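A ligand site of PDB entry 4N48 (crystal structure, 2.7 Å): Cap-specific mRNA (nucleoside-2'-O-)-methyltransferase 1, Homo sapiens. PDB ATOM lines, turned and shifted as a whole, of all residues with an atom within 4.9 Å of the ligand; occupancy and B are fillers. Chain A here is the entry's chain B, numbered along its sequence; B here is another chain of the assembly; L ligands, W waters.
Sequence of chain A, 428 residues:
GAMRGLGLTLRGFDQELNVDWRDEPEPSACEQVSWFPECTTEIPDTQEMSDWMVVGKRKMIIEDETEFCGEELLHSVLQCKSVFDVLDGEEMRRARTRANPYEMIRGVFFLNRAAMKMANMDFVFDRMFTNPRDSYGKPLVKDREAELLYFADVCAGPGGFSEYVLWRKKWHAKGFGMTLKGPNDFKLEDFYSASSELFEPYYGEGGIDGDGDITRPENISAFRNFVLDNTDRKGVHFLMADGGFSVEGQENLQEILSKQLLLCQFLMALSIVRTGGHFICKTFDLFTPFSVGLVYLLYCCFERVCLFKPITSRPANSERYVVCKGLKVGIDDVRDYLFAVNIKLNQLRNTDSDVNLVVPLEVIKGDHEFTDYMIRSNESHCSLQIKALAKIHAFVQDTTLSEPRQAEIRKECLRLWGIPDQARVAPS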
ATOM      1  N   LEU A  78     -17.574   1.179 -12.293  1.00  0.00           N
ATOM      2  CA  LEU A  78     -17.728   0.313 -11.121  1.00  0.00           C
ATOM      3  C   LEU A  78     -19.210   0.115 -10.799  1.00  0.00           C
ATOM      4  O   LEU A  78     -19.632  -0.997 -10.476  1.00  0.00           O
ATOM      5  CB  LEU A  78     -17.008   0.915  -9.920  1.00  0.00           C
ATOM      6  CG  LEU A  78     -15.481   0.854  -9.934  1.00  0.00           C
ATOM      7  CD1 LEU A  78     -14.897   1.705  -8.805  1.00  0.00           C
ATOM      8  CD2 LEU A  78     -15.021  -0.596  -9.809  1.00  0.00           C
ATOM      9  N   LYS A  81     -20.429  -2.211 -13.410  1.00  0.00           N
ATOM     10  CA  LYS A  81     -20.128  -3.599 -13.119  1.00  0.00           C
ATOM     11  C   LYS A  81     -21.073  -4.109 -12.043  1.00  0.00           C
ATOM     12  O   LYS A  81     -21.639  -5.188 -12.152  1.00  0.00           O
ATOM     13  CB  LYS A  81     -18.687  -3.773 -12.643  1.00  0.00           C
ATOM     14  CG  LYS A  81     -17.629  -3.655 -13.734  1.00  0.00           C
ATOM     15  CD  LYS A  81     -16.286  -4.168 -13.248  1.00  0.00           C
ATOM     16  CE  LYS A  81     -15.202  -3.958 -14.291  1.00  0.00           C
ATOM     17  NZ  LYS A  81     -13.936  -4.665 -13.953  1.00  0.00           N
ATOM     18  N   SER A  82     -21.241  -3.299 -10.997  1.00  0.00           N
ATOM     19  CA  SER A  82     -22.029  -3.699  -9.818  1.00  0.00           C
ATOM     20  C   SER A  82     -23.523  -3.878 -10.073  1.00  0.00           C
ATOM     21  O   SER A  82     -24.220  -4.475  -9.255  1.00  0.00           O
ATOM     22  CB  SER A  82     -21.789  -2.734  -8.653  1.00  0.00           C
ATOM     23  OG  SER A  82     -20.531  -2.996  -8.041  1.00  0.00           O
ATOM     24  N   PHE A  84     -24.734  -5.915 -12.046  1.00  0.00           N
ATOM     25  CA  PHE A  84     -24.933  -7.351 -12.186  1.00  0.00           C
ATOM     26  C   PHE A  84     -24.712  -8.113 -10.870  1.00  0.00           C
ATOM     27  O   PHE A  84     -24.656  -9.338 -10.876  1.00  0.00           O
ATOM     28  CB  PHE A  84     -24.015  -7.910 -13.269  1.00  0.00           C
ATOM     29  CG  PHE A  84     -24.041  -7.108 -14.534  1.00  0.00           C
ATOM     30  CD1 PHE A  84     -25.078  -7.251 -15.439  1.00  0.00           C
ATOM     31  CD2 PHE A  84     -23.016  -6.208 -14.819  1.00  0.00           C
ATOM     32  CE1 PHE A  84     -25.101  -6.517 -16.604  1.00  0.00           C
ATOM     33  CE2 PHE A  84     -23.041  -5.462 -15.978  1.00  0.00           C
ATOM     34  CZ  PHE A  84     -24.081  -5.624 -16.878  1.00  0.00           C
ATOM     35  N   ASP A  85     -24.583  -7.378  -9.766  1.00  0.00           N
ATOM     36  CA  ASP A  85     -24.431  -7.997  -8.453  1.00  0.00           C
ATOM     37  C   ASP A  85     -25.698  -8.737  -8.030  1.00  0.00           C
ATOM     38  O   ASP A  85     -25.651  -9.669  -7.217  1.00  0.00           O
ATOM     39  CB  ASP A  85     -24.075  -6.958  -7.389  1.00  0.00           C
ATOM     40  CG  ASP A  85     -22.603  -6.580  -7.425  1.00  0.00           C
ATOM     41  OD1 ASP A  85     -21.780  -7.424  -7.835  1.00  0.00           O
ATOM     42  OD2 ASP A  85     -22.255  -5.451  -7.025  1.00  0.00           O
ATOM     43  N   MET A  92     -27.108 -13.070 -17.473  1.00  0.00           N
ATOM     44  CA  MET A  92     -26.262 -11.945 -17.862  1.00  0.00           C
ATOM     45  C   MET A  92     -25.383 -12.309 -19.052  1.00  0.00           C
ATOM     46  O   MET A  92     -25.237 -11.515 -19.983  1.00  0.00           O
ATOM     47  CB  MET A  92     -25.395 -11.504 -16.689  1.00  0.00           C
ATOM     48  CG  MET A  92     -24.609 -10.229 -16.968  1.00  0.00           C
ATOM     49  SD  MET A  92     -22.852 -10.480 -17.205  1.00  0.00           S
ATOM     50  CE  MET A  92     -22.242 -10.105 -15.565  1.00  0.00           C
ATOM     51  N   ARG A  93     -24.816 -13.505 -19.019  1.00  0.00           N
ATOM     52  CA  ARG A  93     -23.933 -13.974 -20.087  1.00  0.00           C
ATOM     53  C   ARG A  93     -24.692 -14.253 -21.390  1.00  0.00           C
ATOM     54  O   ARG A  93     -24.069 -14.365 -22.454  1.00  0.00           O
ATOM     55  CB  ARG A  93     -23.140 -15.208 -19.645  1.00  0.00           C
ATOM     56  CG  ARG A  93     -22.108 -14.918 -18.576  1.00  0.00           C
ATOM     57  CD  ARG A  93     -21.192 -16.110 -18.312  1.00  0.00           C
ATOM     58  NE  ARG A  93     -21.914 -17.271 -17.799  1.00  0.00           N
ATOM     59  CZ  ARG A  93     -22.172 -17.480 -16.510  1.00  0.00           C
ATOM     60  NH1 ARG A  93     -22.837 -18.571 -16.141  1.00  0.00           N
ATOM     61  NH2 ARG A  93     -21.771 -16.611 -15.600  1.00  0.00           N
ATOM     62  N   ARG A  96     -24.853 -10.781 -22.895  1.00  0.00           N
ATOM     63  CA  ARG A  96     -23.484 -10.520 -23.312  1.00  0.00           C
ATOM     64  C   ARG A  96     -23.235 -11.123 -24.691  1.00  0.00           C
ATOM     65  O   ARG A  96     -22.636 -10.485 -25.559  1.00  0.00           O
ATOM     66  CB  ARG A  96     -22.520 -11.129 -22.296  1.00  0.00           C
ATOM     67  CG  ARG A  96     -21.053 -10.937 -22.610  1.00  0.00           C
ATOM     68  CD  ARG A  96     -20.181 -11.697 -21.616  1.00  0.00           C
ATOM     69  NE  ARG A  96     -20.208 -13.131 -21.868  1.00  0.00           N
ATOM     70  CZ  ARG A  96     -19.417 -14.010 -21.257  1.00  0.00           C
ATOM     71  NH1 ARG A  96     -19.499 -15.302 -21.551  1.00  0.00           N
ATOM     72  NH2 ARG A  96     -18.531 -13.600 -20.357  1.00  0.00           N
ATOM     73  N   GLU A 251     -15.528  -8.977  -7.943  1.00  0.00           N
ATOM     74  CA  GLU A 251     -15.032  -8.687  -9.288  1.00  0.00           C
ATOM     75  C   GLU A 251     -14.359  -7.320  -9.382  1.00  0.00           C
ATOM     76  O   GLU A 251     -13.374  -7.145 -10.085  1.00  0.00           O
ATOM     77  CB  GLU A 251     -16.161  -8.798 -10.315  1.00  0.00           C
ATOM     78  CG  GLU A 251     -16.726 -10.222 -10.508  1.00  0.00           C
ATOM     79  CD  GLU A 251     -17.728 -10.623  -9.442  1.00  0.00           C
ATOM     80  OE1 GLU A 251     -18.119  -9.760  -8.619  1.00  0.00           O
ATOM     81  OE2 GLU A 251     -18.134 -11.803  -9.415  1.00  0.00           O
ATOM     82  N   ASN A 252     -14.905  -6.346  -8.651  1.00  0.00           N
ATOM     83  CA  ASN A 252     -14.419  -4.971  -8.729  1.00  0.00           C
ATOM     84  C   ASN A 252     -12.979  -4.813  -8.255  1.00  0.00           C
ATOM     85  O   ASN A 252     -12.312  -3.843  -8.608  1.00  0.00           O
ATOM     86  CB  ASN A 252     -15.348  -4.018  -7.981  1.00  0.00           C
ATOM     87  CG  ASN A 252     -16.651  -3.774  -8.726  1.00  0.00           C
ATOM     88  OD1 ASN A 252     -16.962  -4.461  -9.691  1.00  0.00           O
ATOM     89  ND2 ASN A 252     -17.408  -2.784  -8.280  1.00  0.00           N
ATOM     90  N   GLN A 254     -10.509  -6.920  -8.936  1.00  0.00           N
ATOM     91  CA  GLN A 254      -9.761  -7.852  -9.770  1.00  0.00           C
ATOM     92  C   GLN A 254      -8.286  -7.479  -9.981  1.00  0.00           C
ATOM     93  O   GLN A 254      -7.405  -8.341  -9.908  1.00  0.00           O
ATOM     94  CB  GLN A 254     -10.464  -7.997 -11.126  1.00  0.00           C
ATOM     95  CG  GLN A 254      -9.737  -8.864 -12.122  1.00  0.00           C
ATOM     96  CD  GLN A 254     -10.418  -8.863 -13.469  1.00  0.00           C
ATOM     97  OE1 GLN A 254     -10.670  -7.793 -14.045  1.00  0.00           O
ATOM     98  NE2 GLN A 254     -10.740 -10.042 -13.966  1.00  0.00           N
ATOM     99  N   PHE A 284      -5.398  -6.315 -16.400  1.00  0.00           N
ATOM    100  CA  PHE A 284      -6.794  -5.954 -16.205  1.00  0.00           C
ATOM    101  C   PHE A 284      -6.851  -4.444 -16.063  1.00  0.00           C
ATOM    102  O   PHE A 284      -6.162  -3.731 -16.797  1.00  0.00           O
ATOM    103  CB  PHE A 284      -7.369  -6.683 -14.989  1.00  0.00           C
ATOM    104  CG  PHE A 284      -7.371  -8.189 -15.144  1.00  0.00           C
ATOM    105  CD1 PHE A 284      -8.304  -8.812 -15.963  1.00  0.00           C
ATOM    106  CD2 PHE A 284      -6.436  -8.980 -14.483  1.00  0.00           C
ATOM    107  CE1 PHE A 284      -8.315 -10.191 -16.115  1.00  0.00           C
ATOM    108  CE2 PHE A 284      -6.441 -10.356 -14.622  1.00  0.00           C
ATOM    109  CZ  PHE A 284      -7.382 -10.969 -15.448  1.00  0.00           C
ATOM    110  N   ARG A 314     -13.579  -9.323 -24.852  1.00  0.00           N
ATOM    111  CA  ARG A 314     -14.966  -8.916 -24.678  1.00  0.00           C
ATOM    112  C   ARG A 314     -15.104  -7.488 -24.164  1.00  0.00           C
ATOM    113  O   ARG A 314     -14.512  -7.135 -23.146  1.00  0.00           O
ATOM    114  CB  ARG A 314     -15.723  -9.903 -23.786  1.00  0.00           C
ATOM    115  CG  ARG A 314     -15.950 -11.277 -24.432  1.00  0.00           C
ATOM    116  CD  ARG A 314     -17.003 -12.074 -23.677  1.00  0.00           C
ATOM    117  NE  ARG A 314     -17.381 -13.302 -24.392  1.00  0.00           N
ATOM    118  CZ  ARG A 314     -16.901 -14.507 -24.111  1.00  0.00           C
ATOM    119  NH1 ARG A 314     -16.015 -14.661 -23.140  1.00  0.00           N
ATOM    120  NH2 ARG A 314     -17.310 -15.551 -24.816  1.00  0.00           N
ATOM    121  N   ALA A 316     -16.994  -5.541 -22.525  1.00  0.00           N
ATOM    122  CA  ALA A 316     -17.513  -5.093 -21.235  1.00  0.00           C
ATOM    123  C   ALA A 316     -16.577  -5.412 -20.072  1.00  0.00           C
ATOM    124  O   ALA A 316     -16.832  -4.996 -18.939  1.00  0.00           O
ATOM    125  CB  ALA A 316     -18.907  -5.668 -20.998  1.00  0.00           C
ATOM    126  N   ASN A 317     -15.493  -6.128 -20.345  1.00  0.00           N
ATOM    127  CA  ASN A 317     -14.533  -6.491 -19.304  1.00  0.00           C
ATOM    128  C   ASN A 317     -13.325  -5.546 -19.201  1.00  0.00           C
ATOM    129  O   ASN A 317     -13.140  -4.660 -20.034  1.00  0.00           O
ATOM    130  CB  ASN A 317     -14.082  -7.954 -19.434  1.00  0.00           C
ATOM    131  CG  ASN A 317     -13.288  -8.234 -20.704  1.00  0.00           C
ATOM    132  OD1 ASN A 317     -12.448  -7.440 -21.128  1.00  0.00           O
ATOM    133  ND2 ASN A 317     -13.559  -9.369 -21.329  1.00  0.00           N
ATOM    134  N   SER A 318     -12.503  -5.762 -18.179  1.00  0.00           N
ATOM    135  CA  SER A 318     -11.357  -4.894 -17.920  1.00  0.00           C
ATOM    136  C   SER A 318     -10.100  -5.473 -18.547  1.00  0.00           C
ATOM    137  O   SER A 318      -8.982  -5.013 -18.275  1.00  0.00           O
ATOM    138  CB  SER A 318     -11.151  -4.721 -16.416  1.00  0.00           C
ATOM    139  OG  SER A 318     -12.269  -4.082 -15.811  1.00  0.00           O
ATOM    140  N   GLN A 385     -15.888   0.564 -22.105  1.00  0.00           N
ATOM    141  CA  GLN A 385     -16.354  -0.504 -21.224  1.00  0.00           C
ATOM    142  C   GLN A 385     -17.701  -0.143 -20.598  1.00  0.00           C
ATOM    143  O   GLN A 385     -18.583  -0.991 -20.485  1.00  0.00           O
ATOM    144  CB  GLN A 385     -15.320  -0.794 -20.144  1.00  0.00           C
ATOM    145  CG  GLN A 385     -15.668  -1.947 -19.214  1.00  0.00           C
ATOM    146  CD  GLN A 385     -14.559  -2.259 -18.221  1.00  0.00           C
ATOM    147  OE1 GLN A 385     -13.596  -1.508 -18.107  1.00  0.00           O
ATOM    148  NE2 GLN A 385     -14.692  -3.371 -17.511  1.00  0.00           N
ATOM    149  N   LEU A 389     -20.991  -2.212 -20.915  1.00  0.00           N
ATOM    150  CA  LEU A 389     -21.619  -2.659 -19.682  1.00  0.00           C
ATOM    151  C   LEU A 389     -23.095  -2.250 -19.665  1.00  0.00           C
ATOM    152  O   LEU A 389     -23.979  -3.053 -19.377  1.00  0.00           O
ATOM    153  CB  LEU A 389     -20.893  -2.086 -18.470  1.00  0.00           C
ATOM    154  CG  LEU A 389     -19.677  -2.909 -18.038  1.00  0.00           C
ATOM    155  CD1 LEU A 389     -18.866  -2.167 -16.978  1.00  0.00           C
ATOM    156  CD2 LEU A 389     -20.129  -4.268 -17.518  1.00  0.00           C
ATOM    157  O5'   G B   1     -12.287 -12.612 -17.938  1.00  0.00           O
ATOM    158  C5'   G B   1     -11.305 -12.222 -18.897  1.00  0.00           C
ATOM    159  C4'   G B   1     -10.185 -13.227 -18.979  1.00  0.00           C
ATOM    160  O4'   G B   1      -9.643 -13.453 -17.649  1.00  0.00           O
ATOM    161  C3'   G B   1     -10.567 -14.605 -19.472  1.00  0.00           C
ATOM    162  O3'   G B   1     -10.594 -14.692 -20.879  1.00  0.00           O
ATOM    163  C2'   G B   1      -9.509 -15.500 -18.833  1.00  0.00           C
ATOM    164  O2'   G B   1      -8.284 -15.412 -19.552  1.00  0.00           O
ATOM    165  C1'   G B   1      -9.326 -14.813 -17.483  1.00  0.00           C
ATOM    166  N9    G B   1     -10.249 -15.362 -16.465  1.00  0.00           N
ATOM    167  C8    G B   1     -11.289 -14.668 -15.891  1.00  0.00           C
ATOM    168  N7    G B   1     -11.974 -15.368 -15.026  1.00  0.00           N
ATOM    169  C5    G B   1     -11.349 -16.604 -15.037  1.00  0.00           C
ATOM    170  C6    G B   1     -11.663 -17.782 -14.308  1.00  0.00           C
ATOM    171  O6    G B   1     -12.567 -17.944 -13.478  1.00  0.00           O
ATOM    172  N1    G B   1     -10.787 -18.814 -14.619  1.00  0.00           N
ATOM    173  C2    G B   1      -9.752 -18.738 -15.517  1.00  0.00           C
ATOM    174  N2    G B   1      -9.020 -19.840 -15.684  1.00  0.00           N
ATOM    175  N3    G B   1      -9.456 -17.641 -16.206  1.00  0.00           N
ATOM    176  C4    G B   1     -10.290 -16.621 -15.920  1.00  0.00           C
ATOM    177  P     A B   2     -11.825 -15.405 -21.628  1.00  0.00           P
ATOM    178  OP1   A B   2     -11.741 -15.025 -23.068  1.00  0.00           O
ATOM    179  OP2   A B   2     -13.081 -15.129 -20.887  1.00  0.00           O
ATOM    180  O5'   A B   2     -11.494 -16.955 -21.510  1.00  0.00           O
ATOM    181  C5'   A B   2     -10.428 -17.544 -22.228  1.00  0.00           C
ATOM    182  C4'   A B   2     -10.294 -19.005 -21.900  1.00  0.00           C
ATOM    183  O4'   A B   2      -9.900 -19.158 -20.515  1.00  0.00           O
ATOM    184  C3'   A B   2     -11.558 -19.833 -22.016  1.00  0.00           C
ATOM    185  O3'   A B   2     -11.862 -20.216 -23.337  1.00  0.00           O
ATOM    186  C2'   A B   2     -11.270 -21.005 -21.094  1.00  0.00           C
ATOM    187  O2'   A B   2     -10.354 -21.909 -21.696  1.00  0.00           O
ATOM    188  C1'   A B   2     -10.544 -20.296 -19.957  1.00  0.00           C
ATOM    189  N9    A B   2     -11.495 -19.831 -18.935  1.00  0.00           N
ATOM    190  C8    A B   2     -12.000 -18.565 -18.789  1.00  0.00           C
ATOM    191  N7    A B   2     -12.850 -18.444 -17.802  1.00  0.00           N
ATOM    192  C5    A B   2     -12.927 -19.725 -17.275  1.00  0.00           C
ATOM    193  C6    A B   2     -13.665 -20.242 -16.208  1.00  0.00           C
ATOM    194  N6    A B   2     -14.494 -19.508 -15.455  1.00  0.00           N
ATOM    195  N1    A B   2     -13.531 -21.559 -15.924  1.00  0.00           N
ATOM    196  C2    A B   2     -12.689 -22.296 -16.682  1.00  0.00           C
ATOM    197  N3    A B   2     -11.936 -21.907 -17.716  1.00  0.00           N
ATOM    198  C4    A B   2     -12.105 -20.598 -17.966  1.00  0.00           C
HETATM  199  P1  LIG L   1     -13.422 -11.638 -17.375  1.00  0.00           P
HETATM  200  O1  LIG L   1     -12.416 -10.587 -16.713  1.00  0.00           O
HETATM  201  O2  LIG L   1     -13.820 -12.628 -16.358  1.00  0.00           O
HETATM  202  O3  LIG L   1     -14.715 -10.890 -17.891  1.00  0.00           O
HETATM  203  P2  LIG L   1     -15.645 -11.598 -18.918  1.00  0.00           P
HETATM  204  O4  LIG L   1     -15.106 -11.441 -20.273  1.00  0.00           O
HETATM  205  O5  LIG L   1     -15.713 -13.027 -18.564  1.00  0.00           O
HETATM  206  O6  LIG L   1     -17.108 -10.949 -18.890  1.00  0.00           O
HETATM  207  P3  LIG L   1     -17.971 -11.003 -17.577  1.00  0.00           P
HETATM  208  O7  LIG L   1     -19.211 -11.867 -17.785  1.00  0.00           O
HETATM  209  O8  LIG L   1     -17.174 -11.583 -16.488  1.00  0.00           O
HETATM  210  O9  LIG L   1     -18.418  -9.499 -17.204  1.00  0.00           O
HETATM  211  C1  LIG L   1     -17.633  -8.442 -17.606  1.00  0.00           C
HETATM  212  C2  LIG L   1     -17.084  -7.569 -16.607  1.00  0.00           C
HETATM  213  O10 LIG L   1     -18.017  -7.436 -15.489  1.00  0.00           O
HETATM  214  C3  LIG L   1     -15.867  -8.142 -16.050  1.00  0.00           C
HETATM  215  O11 LIG L   1     -14.983  -7.109 -15.685  1.00  0.00           O
HETATM  216  C4  LIG L   1     -16.335  -8.878 -14.892  1.00  0.00           C
HETATM  217  O12 LIG L   1     -15.325  -9.041 -13.938  1.00  0.00           O
HETATM  218  C5  LIG L   1     -17.433  -8.025 -14.378  1.00  0.00           C
HETATM  219  N1  LIG L   1     -18.423  -8.806 -13.648  1.00  0.00           N
HETATM  220  C6  LIG L   1     -18.863 -10.034 -13.952  1.00  0.00           C
HETATM  221  N2  LIG L   1     -19.788 -10.420 -13.029  1.00  0.00           N
HETATM  222  C7  LIG L   1     -20.486 -11.706 -13.036  1.00  0.00           C
HETATM  223  C8  LIG L   1     -19.922  -9.420 -12.116  1.00  0.00           C
HETATM  224  C9  LIG L   1     -20.699  -9.211 -10.951  1.00  0.00           C
HETATM  225  O13 LIG L   1     -21.598 -10.170 -10.467  1.00  0.00           O
HETATM  226  N3  LIG L   1     -20.553  -8.037 -10.275  1.00  0.00           N
HETATM  227  C10 LIG L   1     -19.699  -7.078 -10.699  1.00  0.00           C
HETATM  228  N4  LIG L   1     -19.585  -5.826  -9.936  1.00  0.00           N
HETATM  229  N5  LIG L   1     -18.952  -7.249 -11.809  1.00  0.00           N
HETATM  230  C11 LIG L   1     -19.051  -8.396 -12.521  1.00  0.00           C
HETATM  231  O   HOH W   1     -14.838 -11.701 -13.690  1.00  0.00           O
HETATM  232  O   HOH W   2     -13.937 -15.254 -17.738  1.00  0.00           O
HETATM  233  O   HOH W   3     -17.430  -9.313 -21.188  1.00  0.00           O
HETATM  234  O   HOH W   4     -13.855 -12.975 -22.034  1.00  0.00           O
HETATM  235  O   HOH W   5     -13.240  -6.898 -12.911  1.00  0.00           O
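A phosphorus (P1) of the ligand is covalently linked to O5' of G 1 of chain B (1.6 Å).
O4 of the ligand sits at hydrogen-bond distance from ND2 of Asn 317 (2.8 Å).
The side-chain carboxylate of Asp 85 is in hydrogen-bond range of a nitrogen (N3) of the ligand, 2.8 Å away.
N4 of the ligand sits at hydrogen-bond distance from OD1 of Asn 252 (3.0 Å).
The backbone carbonyl oxygen of Lys 81 sits close to a nitrogen (N4) of the ligand (3.1 Å).
O11 of the ligand sits at hydrogen-bond distance from NZ of Lys 81, at 3.2 Å.
The guanidinium group (NH2) of Arg 96 is in salt-bridge range of an oxygen (O7) of the ligand (3.2 Å).
An oxygen (O1) of the ligand lies within hydrogen-bond range of the side-chain amide nitrogen (NE2) of Gln 254 (3.3 Å).
A nitrogen (N3) of the ligand sits at hydrogen-bond distance from the side-chain carboxylate (OE1) of Glu 251 (3.4 Å).
A nitrogen (N4) of the ligand sits close to the backbone NH (N) of Ser 82 (3.2 Å).
The backbone carbonyl oxygen (O) of Phe 84 lies close to an oxygen (O13) of the ligand (3.2 Å).
Residues that only touch the ligand: Met 92 (3.5 Å), Ala 316 (3.5 Å), Ser 318 (3.8 Å) and Arg 314 (3.9 Å).
Hydrophobic or aromatic side chains within 4 Å of the ligand: Met 92.
O of Arg 314 sits close to OD1 of Asn 317 (2.9 Å).
NE2 of Gln 385 lies close to O of Asn 317.
The side-chain amide nitrogen of Asn 252 is in hydrogen-bond range of the side-chain hydroxyl of Ser 82 (3.1 Å).
The side-chain hydroxyl of Ser 318 lies within hydrogen-bond range of the side-chain amino group of Lys 81 (2.6 Å).
The backbone carbonyl oxygen (O) of Leu 78 lies within hydrogen-bond range of the side-chain hydroxyl (OG) of Ser 82.
The backbone carbonyl oxygen (O) of Ala 316 is in hydrogen-bond range of the side-chain amide nitrogen (NE2) of Gln 385 (3.0 Å).
OG of Ser 318 lies within hydrogen-bond range of NE2 of Gln 385 (3.0 Å).
OP2 of A 2 of chain B is in salt-bridge range of NH1 of Arg 314 (3.7 Å).
Water W4 lies within hydrogen-bond range of OP2 of A 2 of chain B (2.6 Å), O4 of the ligand (2.6 Å) and NH1 of Arg 314 (3.0 Å).
Water W2 lies within hydrogen-bond range of an oxygen (O5) of the ligand (3.0 Å), O5' of G 1 of chain B (3.1 Å) and OP2 of A 2 of chain B (3.3 Å).
Water W5 lies within hydrogen-bond range of NZ of Lys 81 (2.6 Å), O of Glu 251 (2.8 Å), OE1 of Gln 254 (2.9 Å) and O12 of the ligand (3.2 Å).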
